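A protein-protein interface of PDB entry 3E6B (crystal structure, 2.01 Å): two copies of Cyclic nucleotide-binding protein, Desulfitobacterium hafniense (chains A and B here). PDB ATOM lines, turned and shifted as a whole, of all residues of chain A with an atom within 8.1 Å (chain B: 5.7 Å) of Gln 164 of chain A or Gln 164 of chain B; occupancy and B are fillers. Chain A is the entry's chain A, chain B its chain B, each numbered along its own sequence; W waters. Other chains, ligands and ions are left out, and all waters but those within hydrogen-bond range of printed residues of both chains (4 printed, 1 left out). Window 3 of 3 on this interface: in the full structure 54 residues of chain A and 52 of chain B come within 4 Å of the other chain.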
ATOM      1  N   PHE A 157      23.195  31.298   9.513  1.00  0.00           N
ATOM      2  CA  PHE A 157      22.106  31.732   8.629  1.00  0.00           C
ATOM      3  C   PHE A 157      22.594  32.683   7.532  1.00  0.00           C
ATOM      4  O   PHE A 157      22.083  32.647   6.403  1.00  0.00           O
ATOM      5  CB  PHE A 157      20.993  32.414   9.413  1.00  0.00           C
ATOM      6  CG  PHE A 157      20.189  31.464  10.261  1.00  0.00           C
ATOM      7  CD1 PHE A 157      19.918  31.743  11.596  1.00  0.00           C
ATOM      8  CD2 PHE A 157      19.663  30.310   9.718  1.00  0.00           C
ATOM      9  CE1 PHE A 157      19.130  30.850  12.390  1.00  0.00           C
ATOM     10  CE2 PHE A 157      18.884  29.422  10.532  1.00  0.00           C
ATOM     11  CZ  PHE A 157      18.650  29.702  11.845  1.00  0.00           C
ATOM     12  N   TYR A 158      23.517  33.567   7.870  1.00  0.00           N
ATOM     13  CA  TYR A 158      24.035  34.475   6.864  1.00  0.00           C
ATOM     14  C   TYR A 158      24.703  33.748   5.702  1.00  0.00           C
ATOM     15  O   TYR A 158      24.421  34.081   4.552  1.00  0.00           O
ATOM     16  CB  TYR A 158      24.943  35.572   7.457  1.00  0.00           C
ATOM     17  CG  TYR A 158      25.514  36.422   6.326  1.00  0.00           C
ATOM     18  CD1 TYR A 158      24.677  37.234   5.537  1.00  0.00           C
ATOM     19  CD2 TYR A 158      26.874  36.314   5.978  1.00  0.00           C
ATOM     20  CE1 TYR A 158      25.186  37.931   4.466  1.00  0.00           C
ATOM     21  CE2 TYR A 158      27.395  37.034   4.951  1.00  0.00           C
ATOM     22  CZ  TYR A 158      26.556  37.823   4.175  1.00  0.00           C
ATOM     23  OH  TYR A 158      27.104  38.521   3.115  1.00  0.00           O
ATOM     24  N   GLU A 159      25.542  32.729   5.969  1.00  0.00           N
ATOM     25  CA  GLU A 159      26.260  31.992   4.899  1.00  0.00           C
ATOM     26  C   GLU A 159      25.287  31.155   4.109  1.00  0.00           C
ATOM     27  O   GLU A 159      25.348  31.037   2.856  1.00  0.00           O
ATOM     28  CB  GLU A 159      27.352  31.083   5.486  1.00  0.00           C
ATOM     29  CG  GLU A 159      28.526  31.885   6.064  1.00  0.00           C
ATOM     30  CD  GLU A 159      29.333  32.612   4.977  1.00  0.00           C
ATOM     31  OE1 GLU A 159      29.815  33.753   5.216  1.00  0.00           O
ATOM     32  OE2 GLU A 159      29.458  32.045   3.879  1.00  0.00           O
ATOM     33  N   LEU A 160      24.319  30.603   4.832  1.00  0.00           N
ATOM     34  CA  LEU A 160      23.306  29.834   4.133  1.00  0.00           C
ATOM     35  C   LEU A 160      22.488  30.696   3.209  1.00  0.00           C
ATOM     36  O   LEU A 160      22.224  30.288   2.081  1.00  0.00           O
ATOM     37  CB  LEU A 160      22.366  29.104   5.097  1.00  0.00           C
ATOM     38  CG  LEU A 160      22.962  27.868   5.760  1.00  0.00           C
ATOM     39  CD1 LEU A 160      21.915  27.243   6.720  1.00  0.00           C
ATOM     40  CD2 LEU A 160      23.490  26.861   4.703  1.00  0.00           C
ATOM     41  N   CYS A 161      22.064  31.853   3.694  1.00  0.00           N
ATOM     42  CA  CYS A 161      21.285  32.786   2.857  1.00  0.00           C
ATOM     43  C   CYS A 161      22.071  33.277   1.649  1.00  0.00           C
ATOM     44  O   CYS A 161      21.567  33.342   0.540  1.00  0.00           O
ATOM     45  CB  CYS A 161      20.815  33.977   3.654  1.00  0.00           C
ATOM     46  SG  CYS A 161      19.438  34.846   2.708  1.00  0.00           S
ATOM     47  N   SER A 162      23.334  33.600   1.838  1.00  0.00           N
ATOM     48  CA  SER A 162      23.989  34.275   0.752  1.00  0.00           C
ATOM     49  C   SER A 162      24.413  33.407  -0.395  1.00  0.00           C
ATOM     50  O   SER A 162      24.598  33.946  -1.516  1.00  0.00           O
ATOM     51  CB  SER A 162      25.054  35.260   1.247  1.00  0.00           C
ATOM     52  OG  SER A 162      26.110  34.612   1.879  1.00  0.00           O
ATOM     53  N   SER A 163      24.489  32.074  -0.171  1.00  0.00           N
ATOM     54  CA  SER A 163      24.774  31.131  -1.252  1.00  0.00           C
ATOM     55  C   SER A 163      23.607  30.240  -1.649  1.00  0.00           C
ATOM     56  O   SER A 163      23.528  29.881  -2.813  1.00  0.00           O
ATOM     57  CB  SER A 163      26.001  30.243  -0.963  1.00  0.00           C
ATOM     58  OG  SER A 163      26.007  29.867   0.410  1.00  0.00           O
ATOM     59  N   GLN A 164      22.733  29.874  -0.715  1.00  0.00           N
ATOM     60  CA  GLN A 164      21.612  28.968  -1.050  1.00  0.00           C
ATOM     61  C   GLN A 164      20.209  29.638  -1.111  1.00  0.00           C
ATOM     62  O   GLN A 164      19.227  28.983  -1.480  1.00  0.00           O
ATOM     63  CB  GLN A 164      21.571  27.782  -0.077  1.00  0.00           C
ATOM     64  CG  GLN A 164      22.963  27.182   0.323  1.00  0.00           C
ATOM     65  CD  GLN A 164      23.729  26.606  -0.842  1.00  0.00           C
ATOM     66  OE1 GLN A 164      23.155  25.984  -1.735  1.00  0.00           O
ATOM     67  NE2 GLN A 164      25.049  26.813  -0.847  1.00  0.00           N
ATOM     68  N   GLY A 165      20.135  30.911  -0.708  1.00  0.00           N
ATOM     69  CA  GLY A 165      18.881  31.691  -0.611  1.00  0.00           C
ATOM     70  C   GLY A 165      18.362  32.076  -1.990  1.00  0.00           C
ATOM     71  O   GLY A 165      19.116  32.568  -2.829  1.00  0.00           O
ATOM     72  N   LYS A 166      17.063  31.883  -2.211  1.00  0.00           N
ATOM     73  CA  LYS A 166      16.416  32.292  -3.480  1.00  0.00           C
ATOM     74  C   LYS A 166      15.593  33.517  -3.207  1.00  0.00           C
ATOM     75  O   LYS A 166      14.840  33.528  -2.243  1.00  0.00           O
ATOM     76  CB  LYS A 166      15.476  31.164  -3.938  1.00  0.00           C
ATOM     77  CG  LYS A 166      16.258  29.815  -4.210  1.00  0.00           C
ATOM     78  CD  LYS A 166      15.218  28.689  -4.403  1.00  0.00           C
ATOM     79  CE  LYS A 166      15.836  27.287  -4.331  1.00  0.00           C
ATOM     80  NZ  LYS A 166      16.558  27.132  -5.576  1.00  0.00           N
ATOM     81  N   ARG A 167      15.713  34.511  -4.068  1.00  0.00           N
ATOM     82  CA  ARG A 167      14.931  35.726  -3.987  1.00  0.00           C
ATOM     83  C   ARG A 167      13.493  35.466  -4.464  1.00  0.00           C
ATOM     84  O   ARG A 167      13.264  35.097  -5.638  1.00  0.00           O
ATOM     85  CB  ARG A 167      15.594  36.808  -4.875  1.00  0.00           C
ATOM     86  CG  ARG A 167      14.990  38.167  -4.717  1.00  0.00           C
ATOM     87  CD  ARG A 167      15.220  38.724  -3.286  1.00  0.00           C
ATOM     88  NE  ARG A 167      14.763  40.121  -3.214  1.00  0.00           N
ATOM     89  CZ  ARG A 167      15.554  41.180  -3.246  1.00  0.00           C
ATOM     90  NH1 ARG A 167      16.895  41.046  -3.322  1.00  0.00           N
ATOM     91  NH2 ARG A 167      15.002  42.378  -3.184  1.00  0.00           N
ATOM     92  N   TYR A 172      14.482  36.330   0.985  1.00  0.00           N
ATOM     93  CA  TYR A 172      15.236  35.143   0.572  1.00  0.00           C
ATOM     94  C   TYR A 172      14.629  33.888   1.220  1.00  0.00           C
ATOM     95  O   TYR A 172      14.337  33.893   2.423  1.00  0.00           O
ATOM     96  CB  TYR A 172      16.775  35.320   0.846  1.00  0.00           C
ATOM     97  CG  TYR A 172      17.390  36.328  -0.122  1.00  0.00           C
ATOM     98  CD1 TYR A 172      17.475  37.678   0.171  1.00  0.00           C
ATOM     99  CD2 TYR A 172      17.841  35.917  -1.382  1.00  0.00           C
ATOM    100  CE1 TYR A 172      18.022  38.598  -0.758  1.00  0.00           C
ATOM    101  CE2 TYR A 172      18.382  36.830  -2.300  1.00  0.00           C
ATOM    102  CZ  TYR A 172      18.462  38.134  -1.991  1.00  0.00           C
ATOM    103  OH  TYR A 172      18.971  38.976  -2.949  1.00  0.00           O
ATOM    104  N   GLU A 173      14.406  32.837   0.427  1.00  0.00           N
ATOM    105  CA  GLU A 173      14.023  31.521   0.954  1.00  0.00           C
ATOM    106  C   GLU A 173      15.155  30.504   0.842  1.00  0.00           C
ATOM    107  O   GLU A 173      15.739  30.329  -0.212  1.00  0.00           O
ATOM    108  CB  GLU A 173      12.785  30.961   0.234  1.00  0.00           C
ATOM    109  CG  GLU A 173      11.504  31.777   0.450  1.00  0.00           C
ATOM    110  CD  GLU A 173      10.255  31.108  -0.161  1.00  0.00           C
ATOM    111  OE1 GLU A 173      10.417  30.113  -0.881  1.00  0.00           O
ATOM    112  OE2 GLU A 173       9.130  31.599   0.086  1.00  0.00           O
ATOM    113  N   ILE A 174      15.474  29.830   1.934  1.00  0.00           N
ATOM    114  CA  ILE A 174      16.445  28.719   1.915  1.00  0.00           C
ATOM    115  C   ILE A 174      15.616  27.469   2.119  1.00  0.00           C
ATOM    116  O   ILE A 174      14.952  27.357   3.143  1.00  0.00           O
ATOM    117  CB  ILE A 174      17.460  28.897   3.117  1.00  0.00           C
ATOM    118  CG1 ILE A 174      18.124  30.288   3.082  1.00  0.00           C
ATOM    119  CG2 ILE A 174      18.461  27.747   3.212  1.00  0.00           C
ATOM    120  CD1 ILE A 174      18.669  30.619   4.403  1.00  0.00           C
ATOM    121  N   THR A 175      15.612  26.550   1.165  1.00  0.00           N
ATOM    122  CA  THR A 175      14.799  25.356   1.251  1.00  0.00           C
ATOM    123  C   THR A 175      15.632  24.269   1.878  1.00  0.00           C
ATOM    124  O   THR A 175      16.496  23.730   1.262  1.00  0.00           O
ATOM    125  CB  THR A 175      14.315  24.868  -0.115  1.00  0.00           C
ATOM    126  OG1 THR A 175      13.607  25.930  -0.761  1.00  0.00           O
ATOM    127  CG2 THR A 175      13.345  23.675   0.103  1.00  0.00           C
ATOM    128  N   MET A 176      15.375  23.990   3.131  1.00  0.00           N
ATOM    129  CA  MET A 176      16.260  23.197   3.913  1.00  0.00           C
ATOM    130  C   MET A 176      15.508  22.963   5.196  1.00  0.00           C
ATOM    131  O   MET A 176      15.089  23.926   5.830  1.00  0.00           O
ATOM    132  CB  MET A 176      17.516  24.017   4.185  1.00  0.00           C
ATOM    133  CG  MET A 176      18.589  23.299   4.874  1.00  0.00           C
ATOM    134  SD  MET A 176      20.026  24.387   4.951  1.00  0.00           S
ATOM    135  CE  MET A 176      21.268  23.129   5.273  1.00  0.00           C
ATOM    136  N   PRO A 177      15.327  21.675   5.567  1.00  0.00           N
ATOM    137  CA  PRO A 177      14.819  21.281   6.864  1.00  0.00           C
ATOM    138  C   PRO A 177      15.964  21.351   7.830  1.00  0.00           C
ATOM    139  O   PRO A 177      16.705  20.409   7.957  1.00  0.00           O
ATOM    140  CB  PRO A 177      14.447  19.790   6.688  1.00  0.00           C
ATOM    141  CG  PRO A 177      14.870  19.386   5.356  1.00  0.00           C
ATOM    142  CD  PRO A 177      15.670  20.506   4.736  1.00  0.00           C
ATOM    143  N   LEU A 178      16.131  22.459   8.511  1.00  0.00           N
ATOM    144  CA  LEU A 178      17.243  22.554   9.415  1.00  0.00           C
ATOM    145  C   LEU A 178      16.596  22.646  10.783  1.00  0.00           C
ATOM    146  O   LEU A 178      16.121  23.714  11.153  1.00  0.00           O
ATOM    147  CB  LEU A 178      18.070  23.792   9.056  1.00  0.00           C
ATOM    148  CG  LEU A 178      19.324  24.123   9.869  1.00  0.00           C
ATOM    149  CD1 LEU A 178      20.328  22.984   9.766  1.00  0.00           C
ATOM    150  CD2 LEU A 178      19.926  25.484   9.399  1.00  0.00           C
ATOM    151  N   ASN A 212      10.385  23.327   6.599  1.00  0.00           N
ATOM    152  CA  ASN A 212      11.124  22.963   5.379  1.00  0.00           C
ATOM    153  C   ASN A 212      11.796  24.181   4.704  1.00  0.00           C
ATOM    154  O   ASN A 212      12.488  24.032   3.691  1.00  0.00           O
ATOM    155  CB  ASN A 212      10.164  22.348   4.371  1.00  0.00           C
ATOM    156  CG  ASN A 212       8.751  22.923   4.483  1.00  0.00           C
ATOM    157  OD1 ASN A 212       8.507  23.937   5.204  1.00  0.00           O
ATOM    158  ND2 ASN A 212       7.779  22.242   3.818  1.00  0.00           N
ATOM    159  N   ILE A 214      13.597  28.319   5.476  1.00  0.00           N
ATOM    160  CA  ILE A 214      13.939  29.456   6.312  1.00  0.00           C
ATOM    161  C   ILE A 214      13.645  30.707   5.483  1.00  0.00           C
ATOM    162  O   ILE A 214      14.101  30.807   4.332  1.00  0.00           O
ATOM    163  CB  ILE A 214      15.424  29.395   6.697  1.00  0.00           C
ATOM    164  CG1 ILE A 214      15.725  28.007   7.332  1.00  0.00           C
ATOM    165  CG2 ILE A 214      15.816  30.617   7.555  1.00  0.00           C
ATOM    166  CD1 ILE A 214      17.161  27.535   7.076  1.00  0.00           C
ATOM    167  N   GLU B 159      24.474  18.121   6.909  1.00  0.00           N
ATOM    168  CA  GLU B 159      23.224  18.865   6.700  1.00  0.00           C
ATOM    169  C   GLU B 159      23.191  19.545   5.332  1.00  0.00           C
ATOM    170  O   GLU B 159      22.167  19.489   4.622  1.00  0.00           O
ATOM    171  CB  GLU B 159      23.004  19.927   7.785  1.00  0.00           C
ATOM    172  CG  GLU B 159      22.763  19.371   9.191  1.00  0.00           C
ATOM    173  CD  GLU B 159      21.565  18.462   9.196  1.00  0.00           C
ATOM    174  OE1 GLU B 159      21.666  17.372   9.795  1.00  0.00           O
ATOM    175  OE2 GLU B 159      20.548  18.810   8.522  1.00  0.00           O
ATOM    176  N   LEU B 160      24.278  20.240   4.978  1.00  0.00           N
ATOM    177  CA  LEU B 160      24.366  20.913   3.677  1.00  0.00           C
ATOM    178  C   LEU B 160      24.223  19.961   2.506  1.00  0.00           C
ATOM    179  O   LEU B 160      23.583  20.300   1.488  1.00  0.00           O
ATOM    180  CB  LEU B 160      25.679  21.690   3.523  1.00  0.00           C
ATOM    181  CG  LEU B 160      25.901  22.949   4.318  1.00  0.00           C
ATOM    182  CD1 LEU B 160      27.383  23.322   4.224  1.00  0.00           C
ATOM    183  CD2 LEU B 160      25.008  24.052   3.752  1.00  0.00           C
ATOM    184  N   CYS B 161      24.839  18.792   2.617  1.00  0.00           N
ATOM    185  CA  CYS B 161      24.842  17.859   1.511  1.00  0.00           C
ATOM    186  C   CYS B 161      23.474  17.178   1.336  1.00  0.00           C
ATOM    187  O   CYS B 161      22.985  16.958   0.215  1.00  0.00           O
ATOM    188  CB  CYS B 161      25.909  16.792   1.711  1.00  0.00           C
ATOM    189  SG  CYS B 161      26.197  15.815   0.269  1.00  0.00           S
ATOM    190  N   SER B 162      22.882  16.804   2.449  1.00  0.00           N
ATOM    191  CA  SER B 162      21.657  16.022   2.388  1.00  0.00           C
ATOM    192  C   SER B 162      20.521  16.899   1.828  1.00  0.00           C
ATOM    193  O   SER B 162      19.708  16.387   1.021  1.00  0.00           O
ATOM    194  CB  SER B 162      21.338  15.406   3.746  1.00  0.00           C
ATOM    195  OG  SER B 162      21.098  16.438   4.667  1.00  0.00           O
ATOM    196  N   SER B 163      20.507  18.199   2.169  1.00  0.00           N
ATOM    197  CA  SER B 163      19.510  19.111   1.590  1.00  0.00           C
ATOM    198  C   SER B 163      19.882  19.906   0.336  1.00  0.00           C
ATOM    199  O   SER B 163      18.991  20.224  -0.446  1.00  0.00           O
ATOM    200  CB  SER B 163      18.841  20.012   2.647  1.00  0.00           C
ATOM    201  OG  SER B 163      19.759  20.912   3.242  1.00  0.00           O
ATOM    202  N   GLN B 164      21.156  20.245   0.121  1.00  0.00           N
ATOM    203  CA  GLN B 164      21.527  21.057  -1.047  1.00  0.00           C
ATOM    204  C   GLN B 164      22.343  20.280  -2.100  1.00  0.00           C
ATOM    205  O   GLN B 164      22.479  20.731  -3.238  1.00  0.00           O
ATOM    206  CB  GLN B 164      22.267  22.353  -0.645  1.00  0.00           C
ATOM    207  CG  GLN B 164      21.701  23.063   0.584  1.00  0.00           C
ATOM    208  CD  GLN B 164      20.321  23.718   0.330  1.00  0.00           C
ATOM    209  OE1 GLN B 164      20.107  24.395  -0.687  1.00  0.00           O
ATOM    210  NE2 GLN B 164      19.381  23.490   1.255  1.00  0.00           N
ATOM    211  N   GLY B 165      22.841  19.112  -1.723  1.00  0.00           N
ATOM    212  CA  GLY B 165      23.650  18.266  -2.618  1.00  0.00           C
ATOM    213  C   GLY B 165      22.923  17.807  -3.863  1.00  0.00           C
ATOM    214  O   GLY B 165      21.809  17.316  -3.784  1.00  0.00           O
ATOM    215  N   LYS B 166      23.573  17.981  -5.013  1.00  0.00           N
ATOM    216  CA  LYS B 166      23.123  17.402  -6.276  1.00  0.00           C
ATOM    217  C   LYS B 166      23.980  16.179  -6.621  1.00  0.00           C
ATOM    218  O   LYS B 166      25.215  16.281  -6.678  1.00  0.00           O
ATOM    219  CB  LYS B 166      23.202  18.471  -7.369  1.00  0.00           C
ATOM    220  CG  LYS B 166      22.629  19.822  -6.901  1.00  0.00           C
ATOM    221  CD  LYS B 166      22.843  20.930  -7.966  1.00  0.00           C
ATOM    222  CE  LYS B 166      23.294  22.283  -7.362  1.00  0.00           C
ATOM    223  NZ  LYS B 166      24.766  22.327  -6.977  1.00  0.00           N
ATOM    224  N   GLU B 173      27.585  17.358  -5.424  1.00  0.00           N
ATOM    225  CA  GLU B 173      28.114  18.698  -5.526  1.00  0.00           C
ATOM    226  C   GLU B 173      27.251  19.702  -4.813  1.00  0.00           C
ATOM    227  O   GLU B 173      26.002  19.761  -5.017  1.00  0.00           O
ATOM    228  CB  GLU B 173      28.307  19.148  -6.986  1.00  0.00           C
ATOM    229  CG  GLU B 173      29.380  18.337  -7.717  1.00  0.00           C
ATOM    230  CD  GLU B 173      29.613  18.805  -9.155  1.00  0.00           C
ATOM    231  OE1 GLU B 173      28.982  19.848  -9.554  1.00  0.00           O
ATOM    232  OE2 GLU B 173      30.439  18.129  -9.861  1.00  0.00           O
ATOM    233  N   ILE B 174      27.917  20.506  -3.988  1.00  0.00           N
ATOM    234  CA  ILE B 174      27.281  21.647  -3.384  1.00  0.00           C
ATOM    235  C   ILE B 174      28.024  22.900  -3.831  1.00  0.00           C
ATOM    236  O   ILE B 174      29.246  22.954  -3.741  1.00  0.00           O
ATOM    237  CB  ILE B 174      27.265  21.611  -1.807  1.00  0.00           C
ATOM    238  CG1 ILE B 174      26.832  20.239  -1.286  1.00  0.00           C
ATOM    239  CG2 ILE B 174      26.317  22.682  -1.301  1.00  0.00           C
ATOM    240  CD1 ILE B 174      27.461  19.887   0.079  1.00  0.00           C
ATOM    241  N   THR B 175      27.268  23.908  -4.266  1.00  0.00           N
ATOM    242  CA  THR B 175      27.806  25.181  -4.684  1.00  0.00           C
ATOM    243  C   THR B 175      27.819  26.217  -3.573  1.00  0.00           C
ATOM    244  O   THR B 175      26.832  26.899  -3.286  1.00  0.00           O
ATOM    245  CB  THR B 175      27.080  25.688  -5.966  1.00  0.00           C
ATOM    246  OG1 THR B 175      26.897  24.575  -6.870  1.00  0.00           O
ATOM    247  CG2 THR B 175      27.924  26.649  -6.620  1.00  0.00           C
ATOM    248  N   MET B 176      28.967  26.362  -2.939  1.00  0.00           N
ATOM    249  CA  MET B 176      29.043  27.149  -1.732  1.00  0.00           C
ATOM    250  C   MET B 176      30.465  27.662  -1.486  1.00  0.00           C
ATOM    251  O   MET B 176      31.365  26.863  -1.139  1.00  0.00           O
ATOM    252  CB  MET B 176      28.605  26.308  -0.544  1.00  0.00           C
ATOM    253  CG  MET B 176      28.662  27.055   0.782  1.00  0.00           C
ATOM    254  SD  MET B 176      27.481  26.275   1.893  1.00  0.00           S
ATOM    255  CE  MET B 176      27.209  27.584   3.095  1.00  0.00           C
HETATM  256  O   HOH W   1      17.669  26.762  -0.888  1.00  0.00           O
HETATM  257  O   HOH W   2      25.235  28.622  -4.552  1.00  0.00           O
HETATM  258  O   HOH W   3      19.255  20.250   6.609  1.00  0.00           O
HETATM  259  O   HOH W   4      18.180  19.118  10.408  1.00  0.00           O
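The side-chain amide nitrogen (NE2) of Gln 164 of chain A is in hydrogen-bond range of the backbone carbonyl oxygen (O) of Thr 175 of chain B, at 3.0 Å.
NE2 of Gln 164 of chain A sits close to SD of Met 176 of chain B (3.7 Å).
O of Thr 175 of chain A lies within hydrogen-bond range of NE2 of Gln 164 of chain B, at 2.9 Å.
The backbone carbonyl oxygen (O) of Glu 159 of chain A sits at hydrogen-bond distance from the side-chain hydroxyl (OG) of Ser 163 of chain A (2.8 Å).
The side-chain hydroxyl (OG) of Ser 163 of chain A is in hydrogen-bond range of the side-chain amide nitrogen (NE2) of Gln 164 of chain A, at 3.4 Å.
The backbone NH (N) of Met 176 of chain A sits at hydrogen-bond distance from the backbone carbonyl oxygen (O) of Asn 212 of chain A, at 2.9 Å.
The backbone carbonyl oxygen (O) of Glu 159 of chain B lies within hydrogen-bond range of the side-chain hydroxyl (OG) of Ser 162 of chain B, at 3.2 Å.
O of Glu 159 of chain B is in hydrogen-bond range of OG of Ser 163 of chain B.
NE2 of Gln 164 of chain B is in hydrogen-bond range of OG of Ser 163 of chain B (3.3 Å).
CE of Met 176 of chain B touches O of Glu 159 of chain A (3.9 Å).
Leu 160 of chain A touches Leu 160 of chain B.
OG of Ser 163 of chain A touches CE of Met 176 of chain B, 3.7 Å away.
OE1 of Gln 164 of chain A touches OE1 of Gln 164 of chain B (3.6 Å).
Glu 159 of chain B touches Met 176 of chain A.
Ser 163 of chain B touches Met 176 of chain A.
Met 176 of chain A touches Gln 164 of chain B.
Ser 163 of chain B touches Pro 177 of chain A.
Of chain A, only Gln 164, Thr 175 and Met 176 come within 4 Å of Gln 164 of chain B.
Gly 165 of chain B touches none of the printed residues of chain A.
Of the printed residues of chain B, Pro 177 of chain A touches Ser 163 (3.8 Å).
Of the printed residues of chain A, Leu 160 of chain B touches Leu 160.
Of the printed residues of chain A, Thr 175 of chain B touches Gln 164.
Printed residues of chain B within 4 Å of Glu 159 of chain A: Met 176.
Ser 162 of chain B touches none of the printed residues of chain A.
Cys 161 of chain A touches none of the printed residues of chain B.
The nearest printed residue of chain B that does not touch Pro 177 of chain A is Glu 159 of chain B (4.2 Å).
Printed residues of chain B that touch a printed residue of chain A: Glu 159, Leu 160, Ser 163, Gln 164, Thr 175 and Met 176.
Of the 20 printed residues of chain A, 7 touch a printed residue of chain B.
Among the printed residues, 11 pairs touch across the chains.
Among the printed residues, no Asp or Glu carboxylate lies within 4 Å of a Lys or Arg side-chain nitrogen of the other chain.
Leu 160 of chain A touches its own counterpart, Leu 160 of chain B.
Ser 163 of chain A touches Met 176 of chain B, and with the chains exchanged Met 176 of chain A touches Ser 163 of chain B.
Gln 164 of chain A touches its own counterpart, Gln 164 of chain B.
Gln 164 of chain A touches Thr 175 of chain B, and with the chains exchanged Thr 175 of chain A touches Gln 164 of chain B.
Positions printed for both chains: 159, 160, 161, 162, 163, 164, 165, 166, 173, 174, 175 and 176.
Of the 11 pairs that touch across the chains among the printed residues, 10 have their exchanged pair printed and touching as well.
Water W2 bridges O of Thr 175 of chain B and O of Ser 163 of chain A.
Water W3 lies within hydrogen-bond range of the side-chain carboxylate of Glu 159 of chain B (2.7 Å), the backbone carbonyl oxygen of Pro 177 of chain A (2.9 Å) and the side-chain hydroxyl of Ser 163 of chain B (3.5 Å).
Water W1 lies within hydrogen-bond range of O of Gln 164 of chain A, N of Thr 175 of chain A and OE1 of Gln 164 of chain B.
Water W4 bridges OE2 of Glu 159 of chain B (3.0 Å) and O of Pro 177 of chain A (3.1 Å).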
